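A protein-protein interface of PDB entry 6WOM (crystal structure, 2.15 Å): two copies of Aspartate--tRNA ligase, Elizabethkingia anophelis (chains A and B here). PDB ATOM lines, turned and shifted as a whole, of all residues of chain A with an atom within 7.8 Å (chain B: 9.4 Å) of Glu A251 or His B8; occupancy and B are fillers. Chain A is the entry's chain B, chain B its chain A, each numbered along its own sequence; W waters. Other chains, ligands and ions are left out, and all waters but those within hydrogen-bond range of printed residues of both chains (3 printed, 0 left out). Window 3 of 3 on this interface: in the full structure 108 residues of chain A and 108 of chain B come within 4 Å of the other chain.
O of Phe B10 sits at hydrogen-bond distance from OG of Ser B30, 2.7 Å away. The backbone NH (N) of Phe A249 sits at hydrogen-bond distance from the backbone carbonyl oxygen (O) of Pro A532 (2.8 Å). The backbone NH of Glu A251 lies within hydrogen-bond range of the side-chain carboxylate of Asp A254 (2.6 Å).
Of the 10 printed residues of chain B, 6 touch a printed residue of chain A. Printed residues of chain B that touch a printed residue of chain A: His B8, Met B9, Phe B10, Arg B11, Ser B30 and Leu B111. Hydrophobic or aromatic side chains of chain B that line the printed part of chain A: Phe B10 and Leu B111. Printed residues of chain A that touch a printed residue of chain B: Phe A249, Val A250, Glu A251 and Pro A532. Among the printed residues, no Asp or Glu carboxylate lies within 4 Å of a Lys or Arg side-chain nitrogen of the other chain.
Water W1 bridges the backbone NH (N) of Phe B10 (2.8 Å) and the backbone carbonyl oxygen (O) of Phe A249 (3.0 Å). Water W3 lies within hydrogen-bond range of OE1 of Glu A251 (3.1 Å) and N of Met B9 (3.4 Å). Water W2 bridges the side-chain carboxylate of Glu A251 (3.5 Å) and the backbone carbonyl oxygen of His B8 (3.5 Å).
OE2 of Glu A251 is in hydrogen-bond range of N of His B8. The backbone NH of Met B9 lies within hydrogen-bond range of the side-chain carboxylate of Glu A251.
No position is printed for both chains. Of the 8 pairs that touch across the chains among the printed residues, none has its exchanged pair printed and touching as well.
Of the printed residues of chain B, Phe A249 touches Phe B10 (3.4 Å), Arg B11 (3.8 Å), Ser B30 (3.4 Å) and Leu B111 (3.9 Å). Of the printed residues of chain B, Glu A251 touches His B8 (2.8 Å) and Met B9 (3.1 Å). Asp A254 touches none of the printed residues of chain B. Asn A477 touches none of the printed residues of chain B. Printed residues of chain B within 4 Å of Pro A532: Phe B10 (3.7 Å). Of chain A, only Glu A251 comes within 4 Å of His B8. Of the printed residues of chain A, Phe B10 touches Phe A249 (3.4 Å), Val A250 (3.7 Å) and Pro A532 (3.7 Å). Printed residues of chain A within 4 Å of Arg B11: Phe A249 (3.8 Å). Thr B28 touches none of the printed residues of chain A. Of the printed residues of chain A, Ser B30 touches Phe A249. The nearest printed residue of chain B that does not touch Phe A249 is Met B9 (6.2 Å).
Among the printed residues, pairs that only touch across the chains: Phe A249 with Phe B10 (3.4 Å), Phe A249 with Arg B11 (3.8 Å), Phe A249 with Ser B30 (3.4 Å), Phe A249 with Leu B111 (3.9 Å), Val A250 with Phe B10 (3.7 Å) and Pro A532 with Phe B10 (3.7 Å).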
ATOM      1  N   MET A 247     -38.364 -18.154   8.028  1.00  0.00           N
ATOM      2  CA  MET A 247     -37.411 -18.689   7.057  1.00  0.00           C
ATOM      3  C   MET A 247     -36.457 -19.659   7.742  1.00  0.00           C
ATOM      4  O   MET A 247     -36.135 -19.491   8.914  1.00  0.00           O
ATOM      5  CB  MET A 247     -36.577 -17.579   6.418  1.00  0.00           C
ATOM      6  CG  MET A 247     -37.433 -16.455   5.836  1.00  0.00           C
ATOM      7  SD  MET A 247     -36.326 -15.108   5.342  1.00  0.00           S
ATOM      8  CE  MET A 247     -35.628 -15.832   3.862  1.00  0.00           C
ATOM      9  N   ALA A 248     -35.977 -20.648   6.992  1.00  0.00           N
ATOM     10  CA  ALA A 248     -35.043 -21.644   7.493  1.00  0.00           C
ATOM     11  C   ALA A 248     -33.645 -21.360   6.958  1.00  0.00           C
ATOM     12  O   ALA A 248     -33.479 -20.693   5.930  1.00  0.00           O
ATOM     13  CB  ALA A 248     -35.484 -23.060   7.084  1.00  0.00           C
ATOM     14  N   PHE A 249     -32.631 -21.875   7.673  1.00  0.00           N
ATOM     15  CA  PHE A 249     -31.227 -21.772   7.247  1.00  0.00           C
ATOM     16  C   PHE A 249     -30.824 -20.332   6.921  1.00  0.00           C
ATOM     17  O   PHE A 249     -30.280 -20.044   5.851  1.00  0.00           O
ATOM     18  CB  PHE A 249     -30.949 -22.697   6.052  1.00  0.00           C
ATOM     19  CG  PHE A 249     -31.240 -24.160   6.344  1.00  0.00           C
ATOM     20  CD1 PHE A 249     -30.410 -24.889   7.190  1.00  0.00           C
ATOM     21  CD2 PHE A 249     -32.333 -24.793   5.781  1.00  0.00           C
ATOM     22  CE1 PHE A 249     -30.680 -26.224   7.465  1.00  0.00           C
ATOM     23  CE2 PHE A 249     -32.604 -26.128   6.051  1.00  0.00           C
ATOM     24  CZ  PHE A 249     -31.763 -26.843   6.901  1.00  0.00           C
ATOM     25  N   VAL A 250     -31.146 -19.409   7.832  1.00  0.00           N
ATOM     26  CA  VAL A 250     -30.864 -17.993   7.617  1.00  0.00           C
ATOM     27  C   VAL A 250     -30.015 -17.456   8.757  1.00  0.00           C
ATOM     28  O   VAL A 250     -30.136 -17.871   9.915  1.00  0.00           O
ATOM     29  CB  VAL A 250     -32.143 -17.123   7.480  1.00  0.00           C
ATOM     30  CG1 VAL A 250     -32.806 -17.342   6.142  1.00  0.00           C
ATOM     31  CG2 VAL A 250     -33.114 -17.379   8.632  1.00  0.00           C
ATOM     32  N   GLU A 251     -29.190 -16.481   8.423  1.00  0.00           N
ATOM     33  CA  GLU A 251     -28.560 -15.634   9.420  1.00  0.00           C
ATOM     34  C   GLU A 251     -29.370 -14.356   9.588  1.00  0.00           C
ATOM     35  O   GLU A 251     -30.197 -14.011   8.738  1.00  0.00           O
ATOM     36  CB  GLU A 251     -27.131 -15.311   8.998  1.00  0.00           C
ATOM     37  CG  GLU A 251     -26.302 -16.573   8.817  1.00  0.00           C
ATOM     38  CD  GLU A 251     -24.922 -16.279   8.268  1.00  0.00           C
ATOM     39  OE1 GLU A 251     -24.735 -16.384   7.029  1.00  0.00           O
ATOM     40  OE2 GLU A 251     -24.032 -15.926   9.078  1.00  0.00           O
ATOM     41  N   GLN A 252     -29.116 -13.648  10.696  1.00  0.00           N
ATOM     42  CA  GLN A 252     -29.775 -12.363  10.920  1.00  0.00           C
ATOM     43  C   GLN A 252     -29.691 -11.478   9.683  1.00  0.00           C
ATOM     44  O   GLN A 252     -30.672 -10.823   9.303  1.00  0.00           O
ATOM     45  CB  GLN A 252     -29.146 -11.655  12.128  1.00  0.00           C
ATOM     46  CG  GLN A 252     -29.598 -10.215  12.302  1.00  0.00           C
ATOM     47  CD  GLN A 252     -29.240  -9.611  13.666  1.00  0.00           C
ATOM     48  OE1 GLN A 252     -29.048  -8.412  13.777  1.00  0.00           O
ATOM     49  NE2 GLN A 252     -29.176 -10.439  14.698  1.00  0.00           N
ATOM     50  N   GLU A 253     -28.523 -11.449   9.044  1.00  0.00           N
ATOM     51  CA  GLU A 253     -28.322 -10.595   7.878  1.00  0.00           C
ATOM     52  C   GLU A 253     -29.237 -11.000   6.728  1.00  0.00           C
ATOM     53  O   GLU A 253     -29.732 -10.141   5.994  1.00  0.00           O
ATOM     54  CB  GLU A 253     -26.846 -10.648   7.459  1.00  0.00           C
ATOM     55  CG  GLU A 253     -26.408  -9.613   6.427  1.00  0.00           C
ATOM     56  CD  GLU A 253     -26.277  -8.199   6.981  1.00  0.00           C
ATOM     57  OE1 GLU A 253     -26.073  -8.036   8.205  1.00  0.00           O
ATOM     58  OE2 GLU A 253     -26.379  -7.241   6.179  1.00  0.00           O
ATOM     59  N   ASP A 254     -29.470 -12.304   6.550  1.00  0.00           N
ATOM     60  CA  ASP A 254     -30.368 -12.758   5.483  1.00  0.00           C
ATOM     61  C   ASP A 254     -31.773 -12.222   5.694  1.00  0.00           C
ATOM     62  O   ASP A 254     -32.391 -11.679   4.769  1.00  0.00           O
ATOM     63  CB  ASP A 254     -30.398 -14.283   5.435  1.00  0.00           C
ATOM     64  CG  ASP A 254     -29.041 -14.869   5.193  1.00  0.00           C
ATOM     65  OD1 ASP A 254     -28.331 -14.355   4.303  1.00  0.00           O
ATOM     66  OD2 ASP A 254     -28.660 -15.779   5.960  1.00  0.00           O
ATOM     67  N   VAL A 255     -32.295 -12.369   6.916  1.00  0.00           N
ATOM     68  CA  VAL A 255     -33.650 -11.908   7.191  1.00  0.00           C
ATOM     69  C   VAL A 255     -33.737 -10.400   6.994  1.00  0.00           C
ATOM     70  O   VAL A 255     -34.699  -9.888   6.401  1.00  0.00           O
ATOM     71  CB  VAL A 255     -34.090 -12.349   8.604  1.00  0.00           C
ATOM     72  CG1 VAL A 255     -35.493 -11.850   8.920  1.00  0.00           C
ATOM     73  CG2 VAL A 255     -34.055 -13.867   8.714  1.00  0.00           C
ATOM     74  N   MET A 256     -32.718  -9.664   7.445  1.00  0.00           N
ATOM     75  CA  MET A 256     -32.764  -8.214   7.295  1.00  0.00           C
ATOM     76  C   MET A 256     -32.745  -7.796   5.829  1.00  0.00           C
ATOM     77  O   MET A 256     -33.504  -6.903   5.424  1.00  0.00           O
ATOM     78  CB  MET A 256     -31.623  -7.557   8.075  1.00  0.00           C
ATOM     79  CG  MET A 256     -31.780  -7.728   9.585  1.00  0.00           C
ATOM     80  SD  MET A 256     -30.379  -7.160  10.566  1.00  0.00           S
ATOM     81  CE  MET A 256     -30.497  -5.376  10.272  1.00  0.00           C
ATOM     82  N   ASN A 257     -31.890  -8.424   5.017  1.00  0.00           N
ATOM     83  CA  ASN A 257     -31.796  -8.045   3.606  1.00  0.00           C
ATOM     84  C   ASN A 257     -33.108  -8.286   2.858  1.00  0.00           C
ATOM     85  O   ASN A 257     -33.532  -7.440   2.062  1.00  0.00           O
ATOM     86  CB  ASN A 257     -30.657  -8.806   2.926  1.00  0.00           C
ATOM     87  CG  ASN A 257     -29.290  -8.313   3.373  1.00  0.00           C
ATOM     88  OD1 ASN A 257     -29.157  -7.208   3.920  1.00  0.00           O
ATOM     89  ND2 ASN A 257     -28.262  -9.102   3.095  1.00  0.00           N
ATOM     90  N   PRO A 461     -23.748 -15.077  18.205  1.00  0.00           N
ATOM     91  CA  PRO A 461     -22.660 -16.063  18.387  1.00  0.00           C
ATOM     92  C   PRO A 461     -21.485 -15.558  19.205  1.00  0.00           C
ATOM     93  O   PRO A 461     -20.967 -16.291  20.059  1.00  0.00           O
ATOM     94  CB  PRO A 461     -22.238 -16.366  16.947  1.00  0.00           C
ATOM     95  CG  PRO A 461     -23.491 -16.157  16.154  1.00  0.00           C
ATOM     96  CD  PRO A 461     -24.190 -14.987  16.803  1.00  0.00           C
ATOM     97  N   ASN A 477     -29.877 -11.966  19.011  1.00  0.00           N
ATOM     98  CA  ASN A 477     -29.948 -12.036  17.557  1.00  0.00           C
ATOM     99  C   ASN A 477     -31.346 -11.587  17.117  1.00  0.00           C
ATOM    100  O   ASN A 477     -32.198 -12.385  16.723  1.00  0.00           O
ATOM    101  CB  ASN A 477     -29.652 -13.462  17.125  1.00  0.00           C
ATOM    102  CG  ASN A 477     -28.585 -13.538  16.102  1.00  0.00           C
ATOM    103  OD1 ASN A 477     -28.411 -12.623  15.300  1.00  0.00           O
ATOM    104  ND2 ASN A 477     -27.785 -14.597  16.178  1.00  0.00           N
ATOM    105  N   TYR A 479     -33.927  -7.926  15.783  1.00  0.00           N
ATOM    106  CA  TYR A 479     -33.888  -6.782  14.887  1.00  0.00           C
ATOM    107  C   TYR A 479     -35.277  -6.165  14.791  1.00  0.00           C
ATOM    108  O   TYR A 479     -36.277  -6.887  14.733  1.00  0.00           O
ATOM    109  CB  TYR A 479     -33.368  -7.209  13.502  1.00  0.00           C
ATOM    110  CG  TYR A 479     -33.809  -8.615  13.137  1.00  0.00           C
ATOM    111  CD1 TYR A 479     -35.052  -8.847  12.544  1.00  0.00           C
ATOM    112  CD2 TYR A 479     -33.011  -9.714  13.427  1.00  0.00           C
ATOM    113  CE1 TYR A 479     -35.476 -10.142  12.225  1.00  0.00           C
ATOM    114  CE2 TYR A 479     -33.421 -11.001  13.113  1.00  0.00           C
ATOM    115  CZ  TYR A 479     -34.655 -11.211  12.520  1.00  0.00           C
ATOM    116  OH  TYR A 479     -35.052 -12.504  12.226  1.00  0.00           O
ATOM    117  N   ILE A 493     -33.615 -14.493  15.313  1.00  0.00           N
ATOM    118  CA  ILE A 493     -33.118 -15.815  14.945  1.00  0.00           C
ATOM    119  C   ILE A 493     -33.337 -16.716  16.158  1.00  0.00           C
ATOM    120  O   ILE A 493     -33.162 -16.285  17.317  1.00  0.00           O
ATOM    121  CB  ILE A 493     -31.631 -15.746  14.515  1.00  0.00           C
ATOM    122  CG1 ILE A 493     -31.424 -14.727  13.389  1.00  0.00           C
ATOM    123  CG2 ILE A 493     -31.073 -17.130  14.069  1.00  0.00           C
ATOM    124  CD1 ILE A 493     -32.292 -14.965  12.148  1.00  0.00           C
ATOM    125  N   PRO A 532     -32.130 -24.637  11.689  1.00  0.00           N
ATOM    126  CA  PRO A 532     -32.008 -23.206  11.990  1.00  0.00           C
ATOM    127  C   PRO A 532     -33.135 -22.459  11.305  1.00  0.00           C
ATOM    128  O   PRO A 532     -33.539 -22.804  10.192  1.00  0.00           O
ATOM    129  CB  PRO A 532     -30.647 -22.826  11.394  1.00  0.00           C
ATOM    130  CG  PRO A 532     -29.912 -24.139  11.224  1.00  0.00           C
ATOM    131  CD  PRO A 532     -30.959 -25.153  10.951  1.00  0.00           C
ATOM    132  N   HIS A 533     -33.677 -21.458  11.996  1.00  0.00           N
ATOM    133  CA  HIS A 533     -34.746 -20.661  11.422  1.00  0.00           C
ATOM    134  C   HIS A 533     -34.824 -19.342  12.173  1.00  0.00           C
ATOM    135  O   HIS A 533     -34.367 -19.217  13.313  1.00  0.00           O
ATOM    136  CB  HIS A 533     -36.108 -21.391  11.455  1.00  0.00           C
ATOM    137  CG  HIS A 533     -36.543 -21.817  12.823  1.00  0.00           C
ATOM    138  ND1 HIS A 533     -37.531 -21.164  13.537  1.00  0.00           N
ATOM    139  CD2 HIS A 533     -36.101 -22.815  13.624  1.00  0.00           C
ATOM    140  CE1 HIS A 533     -37.690 -21.757  14.708  1.00  0.00           C
ATOM    141  NE2 HIS A 533     -36.829 -22.755  14.788  1.00  0.00           N
ATOM    142  N   GLY A 534     -35.382 -18.355  11.494  1.00  0.00           N
ATOM    143  CA  GLY A 534     -35.606 -17.049  12.080  1.00  0.00           C
ATOM    144  C   GLY A 534     -36.763 -16.399  11.361  1.00  0.00           C
ATOM    145  O   GLY A 534     -37.175 -16.837  10.280  1.00  0.00           O
ATOM    146  N   HIS B   8     -21.933 -17.790   9.357  1.00  0.00           N
ATOM    147  CA  HIS B   8     -22.044 -19.056   8.641  1.00  0.00           C
ATOM    148  C   HIS B   8     -23.173 -19.016   7.630  1.00  0.00           C
ATOM    149  O   HIS B   8     -24.329 -19.216   8.006  1.00  0.00           O
ATOM    150  CB  HIS B   8     -22.282 -20.225   9.611  1.00  0.00           C
ATOM    151  N   MET B   9     -22.860 -18.740   6.363  1.00  0.00           N
ATOM    152  CA  MET B   9     -23.789 -19.100   5.304  1.00  0.00           C
ATOM    153  C   MET B   9     -24.099 -20.585   5.419  1.00  0.00           C
ATOM    154  O   MET B   9     -23.192 -21.408   5.539  1.00  0.00           O
ATOM    155  CB  MET B   9     -23.197 -18.797   3.927  1.00  0.00           C
ATOM    156  N   PHE B  10     -25.381 -20.925   5.369  1.00  0.00           N
ATOM    157  CA  PHE B  10     -25.790 -22.317   5.491  1.00  0.00           C
ATOM    158  C   PHE B  10     -25.806 -23.028   4.152  1.00  0.00           C
ATOM    159  O   PHE B  10     -25.740 -24.262   4.122  1.00  0.00           O
ATOM    160  CB  PHE B  10     -27.192 -22.424   6.117  1.00  0.00           C
ATOM    161  CG  PHE B  10     -27.221 -22.168   7.602  1.00  0.00           C
ATOM    162  CD1 PHE B  10     -26.742 -23.105   8.507  1.00  0.00           C
ATOM    163  CD2 PHE B  10     -27.705 -20.969   8.080  1.00  0.00           C
ATOM    164  CE1 PHE B  10     -26.770 -22.844   9.878  1.00  0.00           C
ATOM    165  CE2 PHE B  10     -27.746 -20.700   9.446  1.00  0.00           C
ATOM    166  CZ  PHE B  10     -27.277 -21.633  10.343  1.00  0.00           C
ATOM    167  N   ARG B  11     -25.956 -22.294   3.054  1.00  0.00           N
ATOM    168  CA  ARG B  11     -26.004 -22.921   1.744  1.00  0.00           C
ATOM    169  C   ARG B  11     -25.688 -21.877   0.686  1.00  0.00           C
ATOM    170  O   ARG B  11     -25.978 -20.688   0.850  1.00  0.00           O
ATOM    171  CB  ARG B  11     -27.385 -23.569   1.477  1.00  0.00           C
ATOM    172  CG  ARG B  11     -28.520 -22.588   1.286  1.00  0.00           C
ATOM    173  CD  ARG B  11     -29.890 -23.247   1.572  1.00  0.00           C
ATOM    174  NE  ARG B  11     -30.988 -22.386   1.137  1.00  0.00           N
ATOM    175  CZ  ARG B  11     -32.277 -22.558   1.447  1.00  0.00           C
ATOM    176  NH1 ARG B  11     -32.667 -23.572   2.206  1.00  0.00           N
ATOM    177  NH2 ARG B  11     -33.189 -21.699   0.987  1.00  0.00           N
ATOM    178  N   THR B  12     -25.053 -22.336  -0.386  1.00  0.00           N
ATOM    179  CA  THR B  12     -24.898 -21.557  -1.603  1.00  0.00           C
ATOM    180  C   THR B  12     -25.976 -21.850  -2.631  1.00  0.00           C
ATOM    181  O   THR B  12     -26.158 -21.052  -3.554  1.00  0.00           O
ATOM    182  CB  THR B  12     -23.539 -21.842  -2.251  1.00  0.00           C
ATOM    183  OG1 THR B  12     -23.458 -23.234  -2.593  1.00  0.00           O
ATOM    184  CG2 THR B  12     -22.415 -21.464  -1.318  1.00  0.00           C
ATOM    185  N   THR B  28     -21.965 -25.315  -0.857  1.00  0.00           N
ATOM    186  CA  THR B  28     -22.395 -25.611   0.501  1.00  0.00           C
ATOM    187  C   THR B  28     -23.887 -25.858   0.451  1.00  0.00           C
ATOM    188  O   THR B  28     -24.610 -25.090  -0.185  1.00  0.00           O
ATOM    189  CB  THR B  28     -22.074 -24.451   1.462  1.00  0.00           C
ATOM    190  OG1 THR B  28     -20.657 -24.238   1.467  1.00  0.00           O
ATOM    191  CG2 THR B  28     -22.550 -24.776   2.879  1.00  0.00           C
ATOM    192  N   SER B  30     -27.448 -27.423   2.810  1.00  0.00           N
ATOM    193  CA  SER B  30     -28.066 -27.848   4.062  1.00  0.00           C
ATOM    194  C   SER B  30     -29.418 -28.497   3.761  1.00  0.00           C
ATOM    195  O   SER B  30     -30.077 -28.140   2.777  1.00  0.00           O
ATOM    196  CB  SER B  30     -28.293 -26.648   5.036  1.00  0.00           C
ATOM    197  OG  SER B  30     -27.094 -26.073   5.516  1.00  0.00           O
ATOM    198  N   GLN B  81     -25.320 -29.822   7.404  1.00  0.00           N
ATOM    199  CA  GLN B  81     -24.710 -28.903   6.459  1.00  0.00           C
ATOM    200  C   GLN B  81     -23.430 -29.543   5.947  1.00  0.00           C
ATOM    201  O   GLN B  81     -22.673 -30.114   6.737  1.00  0.00           O
ATOM    202  CB  GLN B  81     -24.419 -27.547   7.117  1.00  0.00           C
ATOM    203  CG  GLN B  81     -23.545 -26.633   6.272  1.00  0.00           C
ATOM    204  CD  GLN B  81     -23.198 -25.331   6.992  1.00  0.00           C
ATOM    205  OE1 GLN B  81     -24.014 -24.772   7.706  1.00  0.00           O
ATOM    206  NE2 GLN B  81     -21.981 -24.857   6.811  1.00  0.00           N
ATOM    207  N   THR B 109     -21.261 -30.759   9.052  1.00  0.00           N
ATOM    208  CA  THR B 109     -21.694 -30.250  10.349  1.00  0.00           C
ATOM    209  C   THR B 109     -23.077 -30.821  10.606  1.00  0.00           C
ATOM    210  O   THR B 109     -23.972 -30.648   9.775  1.00  0.00           O
ATOM    211  CB  THR B 109     -21.735 -28.716  10.370  1.00  0.00           C
ATOM    212  OG1 THR B 109     -20.421 -28.197  10.116  1.00  0.00           O
ATOM    213  CG2 THR B 109     -22.252 -28.209  11.730  1.00  0.00           C
ATOM    214  N   LEU B 111     -26.374 -30.333  12.271  1.00  0.00           N
ATOM    215  CA  LEU B 111     -27.132 -29.233  12.862  1.00  0.00           C
ATOM    216  C   LEU B 111     -28.194 -29.705  13.851  1.00  0.00           C
ATOM    217  O   LEU B 111     -28.474 -29.008  14.827  1.00  0.00           O
ATOM    218  CB  LEU B 111     -27.775 -28.400  11.747  1.00  0.00           C
ATOM    219  CG  LEU B 111     -26.808 -27.740  10.745  1.00  0.00           C
ATOM    220  CD1 LEU B 111     -27.594 -27.205   9.564  1.00  0.00           C
ATOM    221  CD2 LEU B 111     -25.962 -26.602  11.395  1.00  0.00           C
HETATM  222  O   HOH W   1     -27.540 -19.156   4.873  1.00  0.00           O
HETATM  223  O   HOH W   2     -25.072 -18.379  11.301  1.00  0.00           O
HETATM  224  O   HOH W   3     -21.746 -15.541   6.646  1.00  0.00           O
